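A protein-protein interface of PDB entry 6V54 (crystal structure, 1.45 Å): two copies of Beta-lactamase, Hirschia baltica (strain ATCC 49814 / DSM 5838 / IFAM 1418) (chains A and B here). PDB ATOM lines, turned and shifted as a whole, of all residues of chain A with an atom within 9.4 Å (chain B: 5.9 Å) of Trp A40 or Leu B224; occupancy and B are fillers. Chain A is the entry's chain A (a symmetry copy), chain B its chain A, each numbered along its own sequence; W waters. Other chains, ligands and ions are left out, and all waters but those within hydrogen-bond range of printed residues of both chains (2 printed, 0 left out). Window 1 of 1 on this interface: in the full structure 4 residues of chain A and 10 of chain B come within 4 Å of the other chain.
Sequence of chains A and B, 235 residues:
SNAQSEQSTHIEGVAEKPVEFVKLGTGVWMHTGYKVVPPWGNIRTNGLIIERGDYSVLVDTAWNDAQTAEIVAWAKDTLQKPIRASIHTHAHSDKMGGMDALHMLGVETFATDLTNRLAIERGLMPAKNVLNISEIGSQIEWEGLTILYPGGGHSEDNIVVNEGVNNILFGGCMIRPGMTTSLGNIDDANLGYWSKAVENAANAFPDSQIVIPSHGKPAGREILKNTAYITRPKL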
ATOM      1  N   LYS A  35      21.417   5.303  -1.684  1.00  0.00           N
ATOM      2  CA  LYS A  35      22.624   5.565  -2.456  1.00  0.00           C
ATOM      3  C   LYS A  35      23.460   4.301  -2.481  1.00  0.00           C
ATOM      4  O   LYS A  35      23.587   3.624  -1.464  1.00  0.00           O
ATOM      5  CB  LYS A  35      23.461   6.675  -1.783  1.00  0.00           C
ATOM      6  CG  LYS A  35      24.721   7.056  -2.555  1.00  0.00           C
ATOM      7  CD  LYS A  35      25.474   8.190  -1.844  1.00  0.00           C
ATOM      8  CE  LYS A  35      26.757   8.552  -2.566  1.00  0.00           C
ATOM      9  NZ  LYS A  35      27.530   9.610  -1.829  1.00  0.00           N
ATOM     10  N   VAL A  36      24.044   3.984  -3.634  1.00  0.00           N
ATOM     11  CA  VAL A  36      24.897   2.798  -3.756  1.00  0.00           C
ATOM     12  C   VAL A  36      26.319   3.204  -3.415  1.00  0.00           C
ATOM     13  O   VAL A  36      26.920   4.069  -4.085  1.00  0.00           O
ATOM     14  CB  VAL A  36      24.830   2.207  -5.163  1.00  0.00           C
ATOM     15  CG1 VAL A  36      25.727   0.968  -5.233  1.00  0.00           C
ATOM     16  CG2 VAL A  36      23.379   1.886  -5.511  1.00  0.00           C
ATOM     17  N   VAL A  37      26.836   2.616  -2.349  1.00  0.00           N
ATOM     18  CA  VAL A  37      28.193   2.903  -1.885  1.00  0.00           C
ATOM     19  C   VAL A  37      28.941   1.578  -1.771  1.00  0.00           C
ATOM     20  O   VAL A  37      28.680   0.795  -0.845  1.00  0.00           O
ATOM     21  CB  VAL A  37      28.180   3.631  -0.543  1.00  0.00           C
ATOM     22  CG1 VAL A  37      29.595   3.953  -0.165  1.00  0.00           C
ATOM     23  CG2 VAL A  37      27.325   4.950  -0.621  1.00  0.00           C
ATOM     24  N   PRO A  38      29.861   1.269  -2.678  1.00  0.00           N
ATOM     25  CA  PRO A  38      30.650   0.045  -2.520  1.00  0.00           C
ATOM     26  C   PRO A  38      31.465   0.094  -1.245  1.00  0.00           C
ATOM     27  O   PRO A  38      31.926   1.168  -0.822  1.00  0.00           O
ATOM     28  CB  PRO A  38      31.558   0.049  -3.761  1.00  0.00           C
ATOM     29  CG  PRO A  38      30.816   0.851  -4.772  1.00  0.00           C
ATOM     30  CD  PRO A  38      30.101   1.940  -3.973  1.00  0.00           C
ATOM     31  N   PRO A  39      31.747  -1.058  -0.647  1.00  0.00           N
ATOM     32  CA  PRO A  39      31.427  -2.405  -1.118  1.00  0.00           C
ATOM     33  C   PRO A  39      30.041  -2.906  -0.758  1.00  0.00           C
ATOM     34  O   PRO A  39      29.609  -3.906  -1.347  1.00  0.00           O
ATOM     35  CB  PRO A  39      32.465  -3.278  -0.393  1.00  0.00           C
ATOM     36  CG  PRO A  39      32.824  -2.485   0.849  1.00  0.00           C
ATOM     37  CD  PRO A  39      32.691  -1.063   0.500  1.00  0.00           C
ATOM     38  N   TRP A  40      29.374  -2.270   0.215  1.00  0.00           N
ATOM     39  CA  TRP A  40      28.187  -2.898   0.782  1.00  0.00           C
ATOM     40  C   TRP A  40      26.951  -2.613  -0.040  1.00  0.00           C
ATOM     41  O   TRP A  40      25.980  -3.365   0.055  1.00  0.00           O
ATOM     42  CB  TRP A  40      27.996  -2.474   2.248  1.00  0.00           C
ATOM     43  CG  TRP A  40      29.275  -2.611   2.995  1.00  0.00           C
ATOM     44  CD1 TRP A  40      29.884  -1.648   3.719  1.00  0.00           C
ATOM     45  CD2 TRP A  40      30.113  -3.798   3.112  1.00  0.00           C
ATOM     46  NE1 TRP A  40      31.060  -2.120   4.256  1.00  0.00           N
ATOM     47  CE2 TRP A  40      31.223  -3.436   3.905  1.00  0.00           C
ATOM     48  CE3 TRP A  40      30.046  -5.108   2.605  1.00  0.00           C
ATOM     49  CZ2 TRP A  40      32.246  -4.309   4.210  1.00  0.00           C
ATOM     50  CZ3 TRP A  40      31.071  -5.993   2.915  1.00  0.00           C
ATOM     51  CH2 TRP A  40      32.169  -5.583   3.697  1.00  0.00           C
ATOM     52  N   GLY A  41      26.959  -1.561  -0.861  1.00  0.00           N
ATOM     53  CA  GLY A  41      25.833  -1.332  -1.754  1.00  0.00           C
ATOM     54  C   GLY A  41      24.853  -0.292  -1.252  1.00  0.00           C
ATOM     55  O   GLY A  41      25.264   0.705  -0.665  1.00  0.00           O
ATOM     56  N   ASN A  42      23.561  -0.502  -1.494  1.00  0.00           N
ATOM     57  CA  ASN A  42      22.567   0.509  -1.156  1.00  0.00           C
ATOM     58  C   ASN A  42      22.568   0.793   0.332  1.00  0.00           C
ATOM     59  O   ASN A  42      22.609  -0.117   1.166  1.00  0.00           O
ATOM     60  CB  ASN A  42      21.167   0.044  -1.564  1.00  0.00           C
ATOM     61  CG  ASN A  42      20.858   0.382  -3.006  1.00  0.00           C
ATOM     62  OD1 ASN A  42      20.544   1.522  -3.337  1.00  0.00           O
ATOM     63  ND2 ASN A  42      20.965  -0.597  -3.872  1.00  0.00           N
ATOM     64  N   ILE A  43      22.516   2.072   0.674  1.00  0.00           N
ATOM     65  CA  ILE A  43      22.340   2.503   2.056  1.00  0.00           C
ATOM     66  C   ILE A  43      21.192   3.515   2.070  1.00  0.00           C
ATOM     67  O   ILE A  43      21.179   4.451   1.270  1.00  0.00           O
ATOM     68  CB  ILE A  43      23.643   3.083   2.634  1.00  0.00           C
ATOM     69  CG1 ILE A  43      23.373   3.814   3.949  1.00  0.00           C
ATOM     70  CG2 ILE A  43      24.353   3.996   1.653  1.00  0.00           C
ATOM     71  CD1 ILE A  43      24.254   3.431   5.059  1.00  0.00           C
ATOM     72  N   ARG A  44      20.229   3.310   2.956  1.00  0.00           N
ATOM     73  CA  ARG A  44      19.104   4.216   3.116  1.00  0.00           C
ATOM     74  C   ARG A  44      19.491   5.408   3.984  1.00  0.00           C
ATOM     75  O   ARG A  44      20.353   5.321   4.864  1.00  0.00           O
ATOM     76  CB  ARG A  44      17.902   3.512   3.782  1.00  0.00           C
ATOM     77  CG  ARG A  44      18.017   3.329   5.263  1.00  0.00           C
ATOM     78  CD  ARG A  44      16.915   2.447   5.798  1.00  0.00           C
ATOM     79  NE  ARG A  44      15.613   3.104   5.835  1.00  0.00           N
ATOM     80  CZ  ARG A  44      14.483   2.484   6.138  1.00  0.00           C
ATOM     81  NH1 ARG A  44      14.489   1.168   6.374  1.00  0.00           N
ATOM     82  NH2 ARG A  44      13.346   3.154   6.145  1.00  0.00           N
ATOM     83  N   SER A 182      27.792  -2.053  14.892  1.00  0.00           N
ATOM     84  CA  SER A 182      28.612  -1.181  14.052  1.00  0.00           C
ATOM     85  C   SER A 182      28.295   0.279  14.354  1.00  0.00           C
ATOM     86  O   SER A 182      27.151   0.631  14.605  1.00  0.00           O
ATOM     87  CB  SER A 182      28.344  -1.462  12.567  1.00  0.00           C
ATOM     88  OG  SER A 182      27.008  -1.149  12.181  1.00  0.00           O
ATOM     89  N   GLY A 184      28.984   2.752  12.227  1.00  0.00           N
ATOM     90  CA  GLY A 184      28.707   3.509  11.024  1.00  0.00           C
ATOM     91  C   GLY A 184      29.899   4.374  10.652  1.00  0.00           C
ATOM     92  O   GLY A 184      31.048   4.094  11.025  1.00  0.00           O
ATOM     93  N   LEU B 169      24.108 -14.489  -3.857  1.00  0.00           N
ATOM     94  CA  LEU B 169      25.480 -14.766  -3.439  1.00  0.00           C
ATOM     95  C   LEU B 169      25.445 -15.753  -2.283  1.00  0.00           C
ATOM     96  O   LEU B 169      24.886 -15.456  -1.217  1.00  0.00           O
ATOM     97  CB  LEU B 169      26.190 -13.461  -3.039  1.00  0.00           C
ATOM     98  CG  LEU B 169      27.592 -13.650  -2.449  1.00  0.00           C
ATOM     99  CD1 LEU B 169      28.565 -14.324  -3.404  1.00  0.00           C
ATOM    100  CD2 LEU B 169      28.111 -12.280  -2.065  1.00  0.00           C
ATOM    101  N   ILE B 175      30.216 -16.082   5.813  1.00  0.00           N
ATOM    102  CA  ILE B 175      29.281 -15.025   6.165  1.00  0.00           C
ATOM    103  C   ILE B 175      28.511 -15.477   7.392  1.00  0.00           C
ATOM    104  O   ILE B 175      27.898 -16.553   7.380  1.00  0.00           O
ATOM    105  CB  ILE B 175      28.346 -14.701   4.991  1.00  0.00           C
ATOM    106  CG1 ILE B 175      29.172 -14.307   3.756  1.00  0.00           C
ATOM    107  CG2 ILE B 175      27.399 -13.597   5.358  1.00  0.00           C
ATOM    108  CD1 ILE B 175      30.175 -13.134   3.986  1.00  0.00           C
ATOM    109  N   SER B 195      37.981 -10.251   7.321  1.00  0.00           N
ATOM    110  CA  SER B 195      37.164  -9.099   6.930  1.00  0.00           C
ATOM    111  C   SER B 195      37.504  -8.614   5.527  1.00  0.00           C
ATOM    112  O   SER B 195      36.612  -8.157   4.799  1.00  0.00           O
ATOM    113  CB  SER B 195      37.222  -7.975   7.975  1.00  0.00           C
ATOM    114  OG  SER B 195      38.519  -7.404   8.047  1.00  0.00           O
ATOM    115  N   VAL B 198      35.718 -10.883   3.062  1.00  0.00           N
ATOM    116  CA  VAL B 198      34.307 -10.501   2.907  1.00  0.00           C
ATOM    117  C   VAL B 198      34.183  -9.287   1.988  1.00  0.00           C
ATOM    118  O   VAL B 198      33.303  -9.239   1.115  1.00  0.00           O
ATOM    119  CB  VAL B 198      33.635 -10.250   4.273  1.00  0.00           C
ATOM    120  CG1 VAL B 198      32.190  -9.800   4.110  1.00  0.00           C
ATOM    121  CG2 VAL B 198      33.659 -11.500   5.136  1.00  0.00           C
ATOM    122  N   GLU B 199      35.035  -8.272   2.193  1.00  0.00           N
ATOM    123  CA  GLU B 199      35.050  -7.118   1.293  1.00  0.00           C
ATOM    124  C   GLU B 199      35.326  -7.544  -0.145  1.00  0.00           C
ATOM    125  O   GLU B 199      34.674  -7.051  -1.079  1.00  0.00           O
ATOM    126  CB  GLU B 199      36.112  -6.108   1.758  1.00  0.00           C
ATOM    127  CG  GLU B 199      35.722  -5.479   3.049  1.00  0.00           C
ATOM    128  CD  GLU B 199      36.874  -4.815   3.787  1.00  0.00           C
ATOM    129  OE1 GLU B 199      37.987  -4.671   3.220  1.00  0.00           O
ATOM    130  OE2 GLU B 199      36.650  -4.470   4.962  1.00  0.00           O
ATOM    131  N   ALA B 201      34.627 -10.383  -1.609  1.00  0.00           N
ATOM    132  CA  ALA B 201      33.405 -10.972  -2.178  1.00  0.00           C
ATOM    133  C   ALA B 201      32.360  -9.896  -2.474  1.00  0.00           C
ATOM    134  O   ALA B 201      31.672  -9.946  -3.512  1.00  0.00           O
ATOM    135  CB  ALA B 201      32.844 -12.021  -1.218  1.00  0.00           C
ATOM    136  N   ALA B 202      32.161  -8.965  -1.535  1.00  0.00           N
ATOM    137  CA  ALA B 202      31.143  -7.939  -1.732  1.00  0.00           C
ATOM    138  C   ALA B 202      31.471  -7.060  -2.938  1.00  0.00           C
ATOM    139  O   ALA B 202      30.570  -6.678  -3.698  1.00  0.00           O
ATOM    140  CB  ALA B 202      31.063  -7.077  -0.468  1.00  0.00           C
ATOM    141  N   SER B 208      24.328  -8.654  -6.216  1.00  0.00           N
ATOM    142  CA  SER B 208      23.630  -9.664  -5.431  1.00  0.00           C
ATOM    143  C   SER B 208      23.041  -9.068  -4.175  1.00  0.00           C
ATOM    144  O   SER B 208      23.773  -8.692  -3.258  1.00  0.00           O
ATOM    145  CB  SER B 208      24.551 -10.826  -5.108  1.00  0.00           C
ATOM    146  OG  SER B 208      24.800 -11.484  -6.357  1.00  0.00           O
ATOM    147  N   GLN B 209      21.710  -8.994  -4.131  1.00  0.00           N
ATOM    148  CA  GLN B 209      21.001  -8.466  -2.979  1.00  0.00           C
ATOM    149  C   GLN B 209      20.553  -9.553  -2.020  1.00  0.00           C
ATOM    150  O   GLN B 209      20.197  -9.241  -0.879  1.00  0.00           O
ATOM    151  CB  GLN B 209      19.803  -7.611  -3.431  1.00  0.00           C
ATOM    152  CG  GLN B 209      20.212  -6.400  -4.301  1.00  0.00           C
ATOM    153  CD  GLN B 209      21.290  -5.541  -3.642  1.00  0.00           C
ATOM    154  OE1 GLN B 209      21.310  -5.391  -2.427  1.00  0.00           O
ATOM    155  NE2 GLN B 209      22.203  -4.994  -4.444  1.00  0.00           N
ATOM    156  N   VAL B 211      21.795 -12.799   0.066  1.00  0.00           N
ATOM    157  CA  VAL B 211      23.046 -13.381   0.548  1.00  0.00           C
ATOM    158  C   VAL B 211      22.696 -14.552   1.445  1.00  0.00           C
ATOM    159  O   VAL B 211      21.882 -14.405   2.378  1.00  0.00           O
ATOM    160  CB  VAL B 211      23.862 -12.331   1.338  1.00  0.00           C
ATOM    161  CG1 VAL B 211      25.200 -12.933   1.751  1.00  0.00           C
ATOM    162  CG2 VAL B 211      24.132 -11.129   0.460  1.00  0.00           C
ATOM    163  N   GLY B 220      19.994 -10.054   3.264  1.00  0.00           N
ATOM    164  CA  GLY B 220      20.531  -9.142   2.283  1.00  0.00           C
ATOM    165  C   GLY B 220      21.979  -8.782   2.551  1.00  0.00           C
ATOM    166  O   GLY B 220      22.677  -9.426   3.346  1.00  0.00           O
ATOM    167  N   ARG B 221      22.434  -7.734   1.879  1.00  0.00           N
ATOM    168  CA  ARG B 221      23.841  -7.367   1.980  1.00  0.00           C
ATOM    169  C   ARG B 221      24.229  -6.878   3.357  1.00  0.00           C
ATOM    170  O   ARG B 221      25.430  -6.781   3.643  1.00  0.00           O
ATOM    171  CB  ARG B 221      24.199  -6.339   0.912  1.00  0.00           C
ATOM    172  CG  ARG B 221      23.982  -6.895  -0.486  1.00  0.00           C
ATOM    173  CD  ARG B 221      24.434  -5.968  -1.564  1.00  0.00           C
ATOM    174  NE  ARG B 221      25.869  -5.705  -1.595  1.00  0.00           N
ATOM    175  CZ  ARG B 221      26.751  -6.378  -2.340  1.00  0.00           C
ATOM    176  NH1 ARG B 221      26.370  -7.476  -3.022  1.00  0.00           N
ATOM    177  NH2 ARG B 221      28.025  -5.992  -2.372  1.00  0.00           N
ATOM    178  N   GLU B 222      23.260  -6.575   4.218  1.00  0.00           N
ATOM    179  CA  GLU B 222      23.595  -6.217   5.589  1.00  0.00           C
ATOM    180  C   GLU B 222      24.401  -7.285   6.325  1.00  0.00           C
ATOM    181  O   GLU B 222      25.147  -6.947   7.249  1.00  0.00           O
ATOM    182  CB  GLU B 222      22.336  -5.830   6.369  1.00  0.00           C
ATOM    183  CG  GLU B 222      21.464  -7.005   6.792  1.00  0.00           C
ATOM    184  CD  GLU B 222      20.553  -7.559   5.693  1.00  0.00           C
ATOM    185  OE1 GLU B 222      20.501  -6.978   4.573  1.00  0.00           O
ATOM    186  OE2 GLU B 222      19.883  -8.578   5.966  1.00  0.00           O
ATOM    187  N   ILE B 223      24.257  -8.564   5.968  1.00  0.00           N
ATOM    188  CA  ILE B 223      25.043  -9.585   6.642  1.00  0.00           C
ATOM    189  C   ILE B 223      26.468  -9.620   6.104  1.00  0.00           C
ATOM    190  O   ILE B 223      27.356 -10.084   6.814  1.00  0.00           O
ATOM    191  CB  ILE B 223      24.381 -10.985   6.711  1.00  0.00           C
ATOM    192  CG1 ILE B 223      24.228 -11.665   5.351  1.00  0.00           C
ATOM    193  CG2 ILE B 223      22.993 -10.865   7.388  1.00  0.00           C
ATOM    194  CD1 ILE B 223      23.762 -13.108   5.480  1.00  0.00           C
ATOM    195  N   LEU B 224      26.715  -9.138   4.880  1.00  0.00           N
ATOM    196  CA  LEU B 224      28.102  -8.955   4.451  1.00  0.00           C
ATOM    197  C   LEU B 224      28.757  -7.894   5.304  1.00  0.00           C
ATOM    198  O   LEU B 224      29.850  -8.084   5.848  1.00  0.00           O
ATOM    199  CB  LEU B 224      28.174  -8.532   2.973  1.00  0.00           C
ATOM    200  CG  LEU B 224      27.615  -9.546   1.989  1.00  0.00           C
ATOM    201  CD1 LEU B 224      27.579  -8.928   0.591  1.00  0.00           C
ATOM    202  CD2 LEU B 224      28.416 -10.879   1.930  1.00  0.00           C
ATOM    203  N   LYS B 225      28.086  -6.755   5.427  1.00  0.00           N
ATOM    204  CA  LYS B 225      28.623  -5.646   6.195  1.00  0.00           C
ATOM    205  C   LYS B 225      28.802  -5.986   7.661  1.00  0.00           C
ATOM    206  O   LYS B 225      29.825  -5.684   8.239  1.00  0.00           O
ATOM    207  CB  LYS B 225      27.716  -4.422   6.035  1.00  0.00           C
ATOM    208  CG  LYS B 225      28.342  -3.115   6.482  1.00  0.00           C
ATOM    209  CD  LYS B 225      27.333  -1.979   6.394  1.00  0.00           C
ATOM    210  CE  LYS B 225      27.943  -0.665   6.841  1.00  0.00           C
ATOM    211  NZ  LYS B 225      27.286   0.513   6.208  1.00  0.00           N
ATOM    212  N   ASN B 226      27.822  -6.664   8.235  1.00  0.00           N
ATOM    213  CA  ASN B 226      27.939  -7.020   9.641  1.00  0.00           C
ATOM    214  C   ASN B 226      29.066  -8.011   9.843  1.00  0.00           C
ATOM    215  O   ASN B 226      29.836  -7.888  10.808  1.00  0.00           O
ATOM    216  CB  ASN B 226      26.631  -7.606  10.186  1.00  0.00           C
ATOM    217  CG  ASN B 226      26.743  -7.910  11.695  1.00  0.00           C
ATOM    218  OD1 ASN B 226      26.850  -6.968  12.495  1.00  0.00           O
ATOM    219  ND2 ASN B 226      26.764  -9.192  12.088  1.00  0.00           N
ATOM    220  N   THR B 227      29.167  -9.025   8.968  1.00  0.00           N
ATOM    221  CA  THR B 227      30.242  -9.990   9.158  1.00  0.00           C
ATOM    222  C   THR B 227      31.580  -9.287   9.100  1.00  0.00           C
ATOM    223  O   THR B 227      32.459  -9.523   9.929  1.00  0.00           O
ATOM    224  CB  THR B 227      30.197 -11.081   8.091  1.00  0.00           C
ATOM    225  OG1 THR B 227      28.967 -11.825   8.201  1.00  0.00           O
ATOM    226  CG2 THR B 227      31.386 -12.063   8.265  1.00  0.00           C
ATOM    227  N   ALA B 228      31.764  -8.446   8.079  1.00  0.00           N
ATOM    228  CA  ALA B 228      33.057  -7.785   7.938  1.00  0.00           C
ATOM    229  C   ALA B 228      33.393  -6.959   9.172  1.00  0.00           C
ATOM    230  O   ALA B 228      34.570  -6.877   9.573  1.00  0.00           O
ATOM    231  CB  ALA B 228      33.115  -6.911   6.685  1.00  0.00           C
ATOM    232  N   TYR B 229      32.377  -6.324   9.776  1.00  0.00           N
ATOM    233  CA  TYR B 229      32.599  -5.553  10.981  1.00  0.00           C
ATOM    234  C   TYR B 229      32.980  -6.450  12.160  1.00  0.00           C
ATOM    235  O   TYR B 229      33.984  -6.204  12.858  1.00  0.00           O
ATOM    236  CB  TYR B 229      31.353  -4.707  11.317  1.00  0.00           C
ATOM    237  CG  TYR B 229      31.593  -3.870  12.560  1.00  0.00           C
ATOM    238  CD1 TYR B 229      32.465  -2.793  12.514  1.00  0.00           C
ATOM    239  CD2 TYR B 229      31.072  -4.240  13.785  1.00  0.00           C
ATOM    240  CE1 TYR B 229      32.721  -2.051  13.632  1.00  0.00           C
ATOM    241  CE2 TYR B 229      31.337  -3.498  14.921  1.00  0.00           C
ATOM    242  CZ  TYR B 229      32.171  -2.419  14.833  1.00  0.00           C
ATOM    243  OH  TYR B 229      32.464  -1.673  15.952  1.00  0.00           O
ATOM    244  N   ARG B 232      36.524  -7.912  11.861  1.00  0.00           N
ATOM    245  CA  ARG B 232      37.598  -6.963  11.425  1.00  0.00           C
ATOM    246  C   ARG B 232      38.541  -6.635  12.580  1.00  0.00           C
ATOM    247  O   ARG B 232      38.064  -6.231  13.657  1.00  0.00           O
ATOM    248  CB  ARG B 232      36.977  -5.627  10.918  1.00  0.00           C
ATOM    249  CG  ARG B 232      37.946  -4.554  10.315  1.00  0.00           C
ATOM    250  CD  ARG B 232      37.228  -3.275   9.752  1.00  0.00           C
ATOM    251  NE  ARG B 232      36.459  -3.569   8.533  1.00  0.00           N
ATOM    252  CZ  ARG B 232      35.154  -3.348   8.351  1.00  0.00           C
ATOM    253  NH1 ARG B 232      34.405  -2.779   9.293  1.00  0.00           N
ATOM    254  NH2 ARG B 232      34.602  -3.684   7.202  1.00  0.00           N
HETATM  255  O   HOH W   1      22.804  -2.949  -3.111  1.00  0.00           O
HETATM  256  O   HOH W   2      30.074  -3.355  -4.256  1.00  0.00           O
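No position is printed for both chains. Of the 10 pairs that touch across the chains among the printed residues, none has its exchanged pair printed and touching as well.
Water W1 bridges NE2 of Gln B209 and N of Asn A42. Water W2 lies within hydrogen-bond range of the backbone carbonyl oxygen of Pro A39 and the backbone carbonyl oxygen of Ala B202.
Printed residues of chain B that touch a printed residue of chain A: Glu B199, Ala B202, Arg B221, Leu B224, Lys B225, Ala B228, Tyr B229 and Arg B232. Hydrophobic or aromatic side chains of chain A that line the printed part of chain B: Trp A40. Among the printed residues, no Asp or Glu carboxylate lies within 4 Å of a Lys or Arg side-chain nitrogen of the other chain.
Pro A39 touches Ala B202. CH2 of Trp A40 touches CG of Glu B199, 3.6 Å away. Ala B202 touches Trp A40. Trp A40 touches Leu B224 (CZ3 to O, 3.8 Å). Trp A40 touches Lys B225. CH2 of Trp A40 touches CB of Ala B228, at 3.4 Å. Arg B232 touches Trp A40 (NH2 to CZ2, 3.9 Å). Tyr B229 touches Ser A182 (CE2 to CA, 3.7 Å).
The side-chain carboxylate (OE2) of Glu B199 is in salt-bridge range of the guanidinium group (NH2) of Arg B232, at 3.1 Å. O of Ala B202 lies within hydrogen-bond range of NH2 of Arg B221. The backbone carbonyl oxygen (O) of Ser B208 is in hydrogen-bond range of the guanidinium group (NH1) of Arg B221 (2.9 Å).
Printed residues of chain B within 4 Å of Trp A40: Glu B199 (3.6 Å), Ala B202 (3.6 Å), Arg B221 (2.9 Å), Leu B224 (3.8 Å), Lys B225 (3.5 Å), Ala B228 (3.4 Å) and Arg B232 (3.9 Å). Of chain A, only Trp A40 comes within 4 Å of Leu B224. No residue of chain A comes within 4 Å of Ile B223. No residue of chain A comes within 4 Å of Thr B227. Of the printed residues of chain A, Tyr B229 touches Ser A182. Printed residues of chain A within 4 Å of Glu B199: Trp A40. Lys A35 touches none of the printed residues of chain B. Arg A44 touches none of the printed residues of chain B. The nearest residue of chain A that does not touch Leu B224 is Pro A39 (5.8 Å). The nearest printed residue of chain A that does not touch Arg B221 is Gly A41 (4.3 Å).
NH2 of Arg B221 sits at hydrogen-bond distance from O of Pro A39 (2.8 Å). The guanidinium group (NE) of Arg B221 lies within hydrogen-bond range of the backbone carbonyl oxygen (O) of Trp A40, 2.9 Å away.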
